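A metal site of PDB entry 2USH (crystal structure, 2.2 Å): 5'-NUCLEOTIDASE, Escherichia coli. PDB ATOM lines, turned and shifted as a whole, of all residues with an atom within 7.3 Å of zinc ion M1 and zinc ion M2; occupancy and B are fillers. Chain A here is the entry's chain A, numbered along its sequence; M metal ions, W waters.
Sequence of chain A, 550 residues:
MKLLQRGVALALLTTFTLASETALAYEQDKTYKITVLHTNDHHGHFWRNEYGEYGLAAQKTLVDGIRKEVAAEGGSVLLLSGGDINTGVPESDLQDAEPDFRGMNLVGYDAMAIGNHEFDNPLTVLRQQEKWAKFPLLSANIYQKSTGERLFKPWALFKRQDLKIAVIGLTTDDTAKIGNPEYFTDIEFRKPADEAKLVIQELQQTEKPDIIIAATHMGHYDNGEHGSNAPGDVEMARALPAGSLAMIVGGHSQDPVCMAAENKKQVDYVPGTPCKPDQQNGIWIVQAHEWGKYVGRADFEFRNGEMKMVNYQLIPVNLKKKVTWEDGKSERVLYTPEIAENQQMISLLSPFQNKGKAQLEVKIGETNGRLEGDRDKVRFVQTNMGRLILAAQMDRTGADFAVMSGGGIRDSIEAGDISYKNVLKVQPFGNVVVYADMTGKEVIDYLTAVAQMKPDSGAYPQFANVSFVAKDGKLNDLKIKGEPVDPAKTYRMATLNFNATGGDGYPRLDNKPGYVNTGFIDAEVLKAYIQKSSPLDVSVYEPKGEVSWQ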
ATOM      1  N   ASN A  40      -8.236 -23.393 -35.367  1.00  0.00           N
ATOM      2  CA  ASN A  40      -9.000 -23.460 -34.122  1.00  0.00           C
ATOM      3  C   ASN A  40      -9.068 -22.106 -33.458  1.00  0.00           C
ATOM      4  O   ASN A  40      -8.279 -21.230 -33.769  1.00  0.00           O
ATOM      5  CB  ASN A  40      -8.352 -24.435 -33.130  1.00  0.00           C
ATOM      6  CG  ASN A  40      -6.911 -24.103 -32.881  1.00  0.00           C
ATOM      7  OD1 ASN A  40      -6.035 -24.392 -33.720  1.00  0.00           O
ATOM      8  ND2 ASN A  40      -6.642 -23.472 -31.742  1.00  0.00           N
ATOM      9  N   ASP A  41     -10.030 -21.941 -32.556  1.00  0.00           N
ATOM     10  CA  ASP A  41     -10.160 -20.706 -31.793  1.00  0.00           C
ATOM     11  C   ASP A  41     -10.113 -19.435 -32.625  1.00  0.00           C
ATOM     12  O   ASP A  41      -9.345 -18.507 -32.350  1.00  0.00           O
ATOM     13  CB  ASP A  41      -9.076 -20.730 -30.744  1.00  0.00           C
ATOM     14  CG  ASP A  41      -9.218 -21.942 -29.865  1.00  0.00           C
ATOM     15  OD1 ASP A  41      -8.669 -23.021 -30.193  1.00  0.00           O
ATOM     16  OD2 ASP A  41      -9.945 -21.807 -28.866  1.00  0.00           O
ATOM     17  N   HIS A  42     -10.967 -19.452 -33.643  1.00  0.00           N
ATOM     18  CA  HIS A  42     -11.200 -18.389 -34.606  1.00  0.00           C
ATOM     19  C   HIS A  42     -11.645 -17.126 -33.872  1.00  0.00           C
ATOM     20  O   HIS A  42     -11.192 -16.029 -34.175  1.00  0.00           O
ATOM     21  CB  HIS A  42     -12.281 -18.850 -35.596  1.00  0.00           C
ATOM     22  CG  HIS A  42     -12.660 -17.799 -36.596  1.00  0.00           C
ATOM     23  ND1 HIS A  42     -11.785 -17.355 -37.554  1.00  0.00           N
ATOM     24  CD2 HIS A  42     -13.784 -17.059 -36.713  1.00  0.00           C
ATOM     25  CE1 HIS A  42     -12.352 -16.366 -38.230  1.00  0.00           C
ATOM     26  NE2 HIS A  42     -13.562 -16.163 -37.734  1.00  0.00           N
ATOM     27  N   HIS A  43     -12.549 -17.303 -32.913  1.00  0.00           N
ATOM     28  CA  HIS A  43     -13.040 -16.205 -32.098  1.00  0.00           C
ATOM     29  C   HIS A  43     -13.449 -14.850 -32.710  1.00  0.00           C
ATOM     30  O   HIS A  43     -13.019 -13.811 -32.247  1.00  0.00           O
ATOM     31  CB  HIS A  43     -12.066 -15.963 -30.922  1.00  0.00           C
ATOM     32  CG  HIS A  43     -12.078 -17.059 -29.893  1.00  0.00           C
ATOM     33  ND1 HIS A  43     -13.236 -17.486 -29.280  1.00  0.00           N
ATOM     34  CD2 HIS A  43     -11.079 -17.779 -29.339  1.00  0.00           C
ATOM     35  CE1 HIS A  43     -12.954 -18.413 -28.394  1.00  0.00           C
ATOM     36  NE2 HIS A  43     -11.648 -18.623 -28.411  1.00  0.00           N
ATOM     37  N   GLY A  82     -10.926 -26.862 -34.790  1.00  0.00           N
ATOM     38  CA  GLY A  82     -10.938 -27.272 -33.393  1.00  0.00           C
ATOM     39  C   GLY A  82     -11.944 -26.499 -32.528  1.00  0.00           C
ATOM     40  O   GLY A  82     -11.876 -26.575 -31.290  1.00  0.00           O
ATOM     41  N   GLY A  83     -12.855 -25.731 -33.134  1.00  0.00           N
ATOM     42  CA  GLY A  83     -13.849 -25.027 -32.336  1.00  0.00           C
ATOM     43  C   GLY A  83     -13.551 -23.608 -31.874  1.00  0.00           C
ATOM     44  O   GLY A  83     -12.472 -23.080 -32.147  1.00  0.00           O
ATOM     45  N   ASP A  84     -14.465 -23.039 -31.085  1.00  0.00           N
ATOM     46  CA  ASP A  84     -14.395 -21.635 -30.629  1.00  0.00           C
ATOM     47  C   ASP A  84     -14.388 -20.622 -31.779  1.00  0.00           C
ATOM     48  O   ASP A  84     -13.425 -19.901 -32.003  1.00  0.00           O
ATOM     49  CB  ASP A  84     -13.233 -21.371 -29.673  1.00  0.00           C
ATOM     50  CG  ASP A  84     -13.559 -21.752 -28.246  1.00  0.00           C
ATOM     51  OD1 ASP A  84     -14.701 -22.169 -27.993  1.00  0.00           O
ATOM     52  OD2 ASP A  84     -12.701 -21.602 -27.360  1.00  0.00           O
ATOM     53  N   ILE A  85     -15.497 -20.599 -32.508  1.00  0.00           N
ATOM     54  CA  ILE A  85     -15.686 -19.704 -33.624  1.00  0.00           C
ATOM     55  C   ILE A  85     -16.278 -18.441 -33.003  1.00  0.00           C
ATOM     56  O   ILE A  85     -16.003 -17.325 -33.438  1.00  0.00           O
ATOM     57  CB  ILE A  85     -16.714 -20.313 -34.628  1.00  0.00           C
ATOM     58  CG1 ILE A  85     -16.254 -21.727 -34.985  1.00  0.00           C
ATOM     59  CG2 ILE A  85     -16.885 -19.415 -35.851  1.00  0.00           C
ATOM     60  CD1 ILE A  85     -14.846 -21.818 -35.506  1.00  0.00           C
ATOM     61  N   ASN A  86     -17.104 -18.645 -31.975  1.00  0.00           N
ATOM     62  CA  ASN A  86     -17.776 -17.594 -31.215  1.00  0.00           C
ATOM     63  C   ASN A  86     -16.907 -16.838 -30.233  1.00  0.00           C
ATOM     64  O   ASN A  86     -15.963 -17.385 -29.661  1.00  0.00           O
ATOM     65  CB  ASN A  86     -18.963 -18.157 -30.387  1.00  0.00           C
ATOM     66  CG  ASN A  86     -20.187 -18.520 -31.232  1.00  0.00           C
ATOM     67  OD1 ASN A  86     -21.036 -17.671 -31.479  1.00  0.00           O
ATOM     68  ND2 ASN A  86     -20.316 -19.777 -31.639  1.00  0.00           N
ATOM     69  N   THR A  87     -17.276 -15.572 -30.034  1.00  0.00           N
ATOM     70  CA  THR A  87     -16.684 -14.676 -29.030  1.00  0.00           C
ATOM     71  C   THR A  87     -15.275 -14.176 -29.240  1.00  0.00           C
ATOM     72  O   THR A  87     -14.347 -14.951 -29.251  1.00  0.00           O
ATOM     73  CB  THR A  87     -16.736 -15.355 -27.673  1.00  0.00           C
ATOM     74  OG1 THR A  87     -18.098 -15.764 -27.414  1.00  0.00           O
ATOM     75  CG2 THR A  87     -16.265 -14.412 -26.568  1.00  0.00           C
ATOM     76  N   GLY A 115     -16.624 -25.957 -29.412  1.00  0.00           N
ATOM     77  CA  GLY A 115     -15.803 -25.413 -28.341  1.00  0.00           C
ATOM     78  C   GLY A 115     -16.583 -24.907 -27.136  1.00  0.00           C
ATOM     79  O   GLY A 115     -17.807 -24.828 -27.149  1.00  0.00           O
ATOM     80  N   ASN A 116     -15.880 -24.558 -26.064  1.00  0.00           N
ATOM     81  CA  ASN A 116     -16.571 -24.079 -24.897  1.00  0.00           C
ATOM     82  C   ASN A 116     -17.290 -22.750 -25.173  1.00  0.00           C
ATOM     83  O   ASN A 116     -18.346 -22.493 -24.615  1.00  0.00           O
ATOM     84  CB  ASN A 116     -15.596 -23.983 -23.704  1.00  0.00           C
ATOM     85  CG  ASN A 116     -14.448 -23.030 -23.961  1.00  0.00           C
ATOM     86  OD1 ASN A 116     -13.749 -23.130 -24.959  1.00  0.00           O
ATOM     87  ND2 ASN A 116     -14.232 -22.098 -23.034  1.00  0.00           N
ATOM     88  N   HIS A 117     -16.738 -21.914 -26.044  1.00  0.00           N
ATOM     89  CA  HIS A 117     -17.401 -20.640 -26.348  1.00  0.00           C
ATOM     90  C   HIS A 117     -18.600 -20.690 -27.312  1.00  0.00           C
ATOM     91  O   HIS A 117     -19.146 -19.635 -27.667  1.00  0.00           O
ATOM     92  CB  HIS A 117     -16.403 -19.556 -26.815  1.00  0.00           C
ATOM     93  CG  HIS A 117     -15.528 -19.042 -25.710  1.00  0.00           C
ATOM     94  ND1 HIS A 117     -15.955 -18.078 -24.819  1.00  0.00           N
ATOM     95  CD2 HIS A 117     -14.291 -19.415 -25.289  1.00  0.00           C
ATOM     96  CE1 HIS A 117     -15.042 -17.898 -23.886  1.00  0.00           C
ATOM     97  NE2 HIS A 117     -14.024 -18.689 -24.152  1.00  0.00           N
ATOM     98  N   THR A 172     -14.264 -29.965 -24.214  1.00  0.00           N
ATOM     99  CA  THR A 172     -13.804 -29.888 -22.822  1.00  0.00           C
ATOM    100  C   THR A 172     -14.971 -29.859 -21.849  1.00  0.00           C
ATOM    101  O   THR A 172     -15.960 -29.141 -22.030  1.00  0.00           O
ATOM    102  CB  THR A 172     -12.903 -28.631 -22.551  1.00  0.00           C
ATOM    103  OG1 THR A 172     -12.492 -28.654 -21.178  1.00  0.00           O
ATOM    104  CG2 THR A 172     -13.647 -27.340 -22.835  1.00  0.00           C
ATOM    105  N   THR A 175     -16.332 -26.632 -19.821  1.00  0.00           N
ATOM    106  CA  THR A 175     -17.273 -25.687 -20.375  1.00  0.00           C
ATOM    107  C   THR A 175     -18.271 -25.218 -19.355  1.00  0.00           C
ATOM    108  O   THR A 175     -18.632 -24.067 -19.380  1.00  0.00           O
ATOM    109  CB  THR A 175     -17.972 -26.284 -21.598  1.00  0.00           C
ATOM    110  OG1 THR A 175     -16.975 -26.503 -22.607  1.00  0.00           O
ATOM    111  CG2 THR A 175     -19.078 -25.334 -22.130  1.00  0.00           C
ATOM    112  N   HIS A 217     -11.737 -29.986 -28.568  1.00  0.00           N
ATOM    113  CA  HIS A 217     -11.548 -28.654 -28.017  1.00  0.00           C
ATOM    114  C   HIS A 217     -11.246 -28.866 -26.523  1.00  0.00           C
ATOM    115  O   HIS A 217     -12.073 -28.596 -25.654  1.00  0.00           O
ATOM    116  CB  HIS A 217     -12.788 -27.825 -28.231  1.00  0.00           C
ATOM    117  CG  HIS A 217     -12.553 -26.395 -27.943  1.00  0.00           C
ATOM    118  ND1 HIS A 217     -12.036 -25.550 -28.899  1.00  0.00           N
ATOM    119  CD2 HIS A 217     -12.617 -25.692 -26.793  1.00  0.00           C
ATOM    120  CE1 HIS A 217     -11.777 -24.384 -28.340  1.00  0.00           C
ATOM    121  NE2 HIS A 217     -12.107 -24.449 -27.061  1.00  0.00           N
ATOM    122  N   MET A 218     -10.027 -29.353 -26.252  1.00  0.00           N
ATOM    123  CA  MET A 218      -9.622 -29.724 -24.890  1.00  0.00           C
ATOM    124  C   MET A 218      -8.328 -29.080 -24.376  1.00  0.00           C
ATOM    125  O   MET A 218      -8.170 -28.912 -23.176  1.00  0.00           O
ATOM    126  CB  MET A 218      -9.549 -31.265 -24.833  1.00  0.00           C
ATOM    127  CG  MET A 218     -10.913 -31.947 -25.174  1.00  0.00           C
ATOM    128  SD  MET A 218     -10.833 -33.740 -25.459  1.00  0.00           S
ATOM    129  CE  MET A 218      -9.636 -34.288 -24.235  1.00  0.00           C
ATOM    130  N   GLY A 251      -7.459 -27.621 -29.888  1.00  0.00           N
ATOM    131  CA  GLY A 251      -7.745 -26.209 -29.669  1.00  0.00           C
ATOM    132  C   GLY A 251      -7.903 -25.895 -28.192  1.00  0.00           C
ATOM    133  O   GLY A 251      -7.431 -26.649 -27.328  1.00  0.00           O
ATOM    134  N   HIS A 252      -8.526 -24.765 -27.906  1.00  0.00           N
ATOM    135  CA  HIS A 252      -8.840 -24.340 -26.556  1.00  0.00           C
ATOM    136  C   HIS A 252      -7.701 -23.708 -25.785  1.00  0.00           C
ATOM    137  O   HIS A 252      -7.847 -22.603 -25.263  1.00  0.00           O
ATOM    138  CB  HIS A 252      -9.421 -25.508 -25.741  1.00  0.00           C
ATOM    139  CG  HIS A 252      -9.931 -25.098 -24.389  1.00  0.00           C
ATOM    140  ND1 HIS A 252     -10.853 -24.095 -24.228  1.00  0.00           N
ATOM    141  CD2 HIS A 252      -9.651 -25.559 -23.149  1.00  0.00           C
ATOM    142  CE1 HIS A 252     -11.119 -23.947 -22.945  1.00  0.00           C
ATOM    143  NE2 HIS A 252     -10.407 -24.816 -22.272  1.00  0.00           N
ATOM    144  N   SER A 253      -6.592 -24.420 -25.661  1.00  0.00           N
ATOM    145  CA  SER A 253      -5.434 -23.861 -24.984  1.00  0.00           C
ATOM    146  C   SER A 253      -4.860 -22.727 -25.854  1.00  0.00           C
ATOM    147  O   SER A 253      -4.215 -21.844 -25.345  1.00  0.00           O
ATOM    148  CB  SER A 253      -4.366 -24.938 -24.701  1.00  0.00           C
ATOM    149  OG  SER A 253      -3.888 -25.605 -25.864  1.00  0.00           O
ATOM    150  N   GLN A 254      -5.101 -22.773 -27.170  1.00  0.00           N
ATOM    151  CA  GLN A 254      -4.642 -21.767 -28.117  1.00  0.00           C
ATOM    152  C   GLN A 254      -3.150 -21.558 -28.242  1.00  0.00           C
ATOM    153  O   GLN A 254      -2.656 -20.439 -28.160  1.00  0.00           O
ATOM    154  CB  GLN A 254      -5.341 -20.434 -27.840  1.00  0.00           C
ATOM    155  CG  GLN A 254      -6.849 -20.575 -27.989  1.00  0.00           C
ATOM    156  CD  GLN A 254      -7.606 -19.298 -27.682  1.00  0.00           C
ATOM    157  OE1 GLN A 254      -8.739 -19.336 -27.200  1.00  0.00           O
ATOM    158  NE2 GLN A 254      -6.984 -18.156 -27.977  1.00  0.00           N
ATOM    159  N   HIS A 289      -2.785 -22.501 -32.814  1.00  0.00           N
ATOM    160  CA  HIS A 289      -2.796 -21.263 -32.086  1.00  0.00           C
ATOM    161  C   HIS A 289      -4.182 -20.602 -31.986  1.00  0.00           C
ATOM    162  O   HIS A 289      -5.030 -21.073 -31.223  1.00  0.00           O
ATOM    163  CB  HIS A 289      -1.786 -20.334 -32.754  1.00  0.00           C
ATOM    164  CG  HIS A 289      -1.527 -19.082 -32.000  1.00  0.00           C
ATOM    165  ND1 HIS A 289      -1.588 -19.017 -30.627  1.00  0.00           N
ATOM    166  CD2 HIS A 289      -1.154 -17.846 -32.422  1.00  0.00           C
ATOM    167  CE1 HIS A 289      -1.260 -17.794 -30.228  1.00  0.00           C
ATOM    168  NE2 HIS A 289      -0.986 -17.074 -31.303  1.00  0.00           N
ATOM    169  N   GLU A 290      -4.457 -19.536 -32.730  1.00  0.00           N
ATOM    170  CA  GLU A 290      -5.755 -18.915 -32.570  1.00  0.00           C
ATOM    171  C   GLU A 290      -5.965 -17.857 -33.644  1.00  0.00           C
ATOM    172  O   GLU A 290      -5.030 -17.478 -34.331  1.00  0.00           O
ATOM    173  CB  GLU A 290      -5.805 -18.180 -31.215  1.00  0.00           C
ATOM    174  CG  GLU A 290      -4.859 -16.962 -31.266  1.00  0.00           C
ATOM    175  CD  GLU A 290      -4.558 -16.334 -29.932  1.00  0.00           C
ATOM    176  OE1 GLU A 290      -4.920 -16.911 -28.890  1.00  0.00           O
ATOM    177  OE2 GLU A 290      -3.933 -15.262 -29.941  1.00  0.00           O
ATOM    178  N   TRP A 291      -7.228 -17.396 -33.738  1.00  0.00           N
ATOM    179  CA  TRP A 291      -7.663 -16.301 -34.611  1.00  0.00           C
ATOM    180  C   TRP A 291      -7.426 -16.327 -36.122  1.00  0.00           C
ATOM    181  O   TRP A 291      -7.445 -15.269 -36.760  1.00  0.00           O
ATOM    182  CB  TRP A 291      -7.066 -14.981 -34.090  1.00  0.00           C
ATOM    183  CG  TRP A 291      -7.388 -14.668 -32.642  1.00  0.00           C
ATOM    184  CD1 TRP A 291      -8.207 -15.366 -31.798  1.00  0.00           C
ATOM    185  CD2 TRP A 291      -6.839 -13.576 -31.867  1.00  0.00           C
ATOM    186  NE1 TRP A 291      -8.206 -14.783 -30.552  1.00  0.00           N
ATOM    187  CE2 TRP A 291      -7.376 -13.687 -30.569  1.00  0.00           C
ATOM    188  CE3 TRP A 291      -5.951 -12.521 -32.151  1.00  0.00           C
ATOM    189  CZ2 TRP A 291      -7.048 -12.772 -29.535  1.00  0.00           C
ATOM    190  CZ3 TRP A 291      -5.628 -11.612 -31.132  1.00  0.00           C
ATOM    191  CH2 TRP A 291      -6.186 -11.749 -29.835  1.00  0.00           C
ATOM    192  N   THR A 518     -10.304 -16.796 -19.327  1.00  0.00           N
ATOM    193  CA  THR A 518     -11.716 -17.023 -19.704  1.00  0.00           C
ATOM    194  C   THR A 518     -12.004 -16.871 -21.176  1.00  0.00           C
ATOM    195  O   THR A 518     -13.014 -17.348 -21.656  1.00  0.00           O
ATOM    196  CB  THR A 518     -12.670 -16.066 -19.003  1.00  0.00           C
ATOM    197  OG1 THR A 518     -12.382 -14.722 -19.443  1.00  0.00           O
ATOM    198  CG2 THR A 518     -12.500 -16.156 -17.491  1.00  0.00           C
ATOM    199  N   GLY A 519     -11.131 -16.193 -21.899  1.00  0.00           N
ATOM    200  CA  GLY A 519     -11.434 -15.994 -23.294  1.00  0.00           C
ATOM    201  C   GLY A 519     -12.439 -14.852 -23.475  1.00  0.00           C
ATOM    202  O   GLY A 519     -12.833 -14.593 -24.601  1.00  0.00           O
HETATM  203 ZN    ZN M   1     -10.730 -20.384 -27.515  1.00  0.00          ZN
HETATM  204 ZN    ZN M   2     -11.919 -22.914 -25.706  1.00  0.00          ZN
HETATM  205  O   HOH W   1     -10.672 -21.186 -25.634  1.00  0.00           O
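Zinc ion M2 is bound by the side-chain amide oxygen (OD1) of Asn 116 (2.0 Å), a ring nitrogen (NE2) of His 217 (2.1 Å), water W1 (2.1 Å), a ring nitrogen (ND1) of His 252 (2.2 Å) and the side-chain carboxylate (OD2) of Asp 84 (2.3 Å).
Zinc ion M2 has five donor atoms within binding distance.
Of the 26 residues printed, 4 come within 4 Å of zinc ion M1.
Zinc ion M1 is bound by water W1 (2.0 Å), the side-chain carboxylate of Asp 41 (2.1 Å), a ring nitrogen (NE2) of His 43 (2.2 Å), the side-chain amide oxygen of Gln 254 (2.3 Å) and the side-chain carboxylate of Asp 84 (2.3 Å).
The backbone NH (N) of Thr 172 is in hydrogen-bond range of the backbone carbonyl oxygen (O) of His 217.
The backbone carbonyl oxygen (O) of Gly 82 sits at hydrogen-bond distance from a ring nitrogen (ND1) of His 217 (2.6 Å).
The backbone carbonyl oxygen of Gly 83 lies within hydrogen-bond range of the backbone NH of Asp 41 (2.7 Å).
OD1 of Asp 41 lies within hydrogen-bond range of ND2 of Asn 40, at 2.6 Å.
A ring nitrogen (ND1) of His 43 lies within hydrogen-bond range of the backbone carbonyl oxygen (O) of Thr 87, at 2.8 Å.
The side-chain carboxylate (OD1) of Asp 84 is in hydrogen-bond range of the backbone NH (N) of His 117, at 2.8 Å.
The side-chain amide nitrogen (NE2) of Gln 254 sits at hydrogen-bond distance from the side-chain carboxylate (OE1) of Glu 290 (2.6 Å).
The backbone carbonyl oxygen of Gln 254 sits at hydrogen-bond distance from a ring nitrogen (ND1) of His 289.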
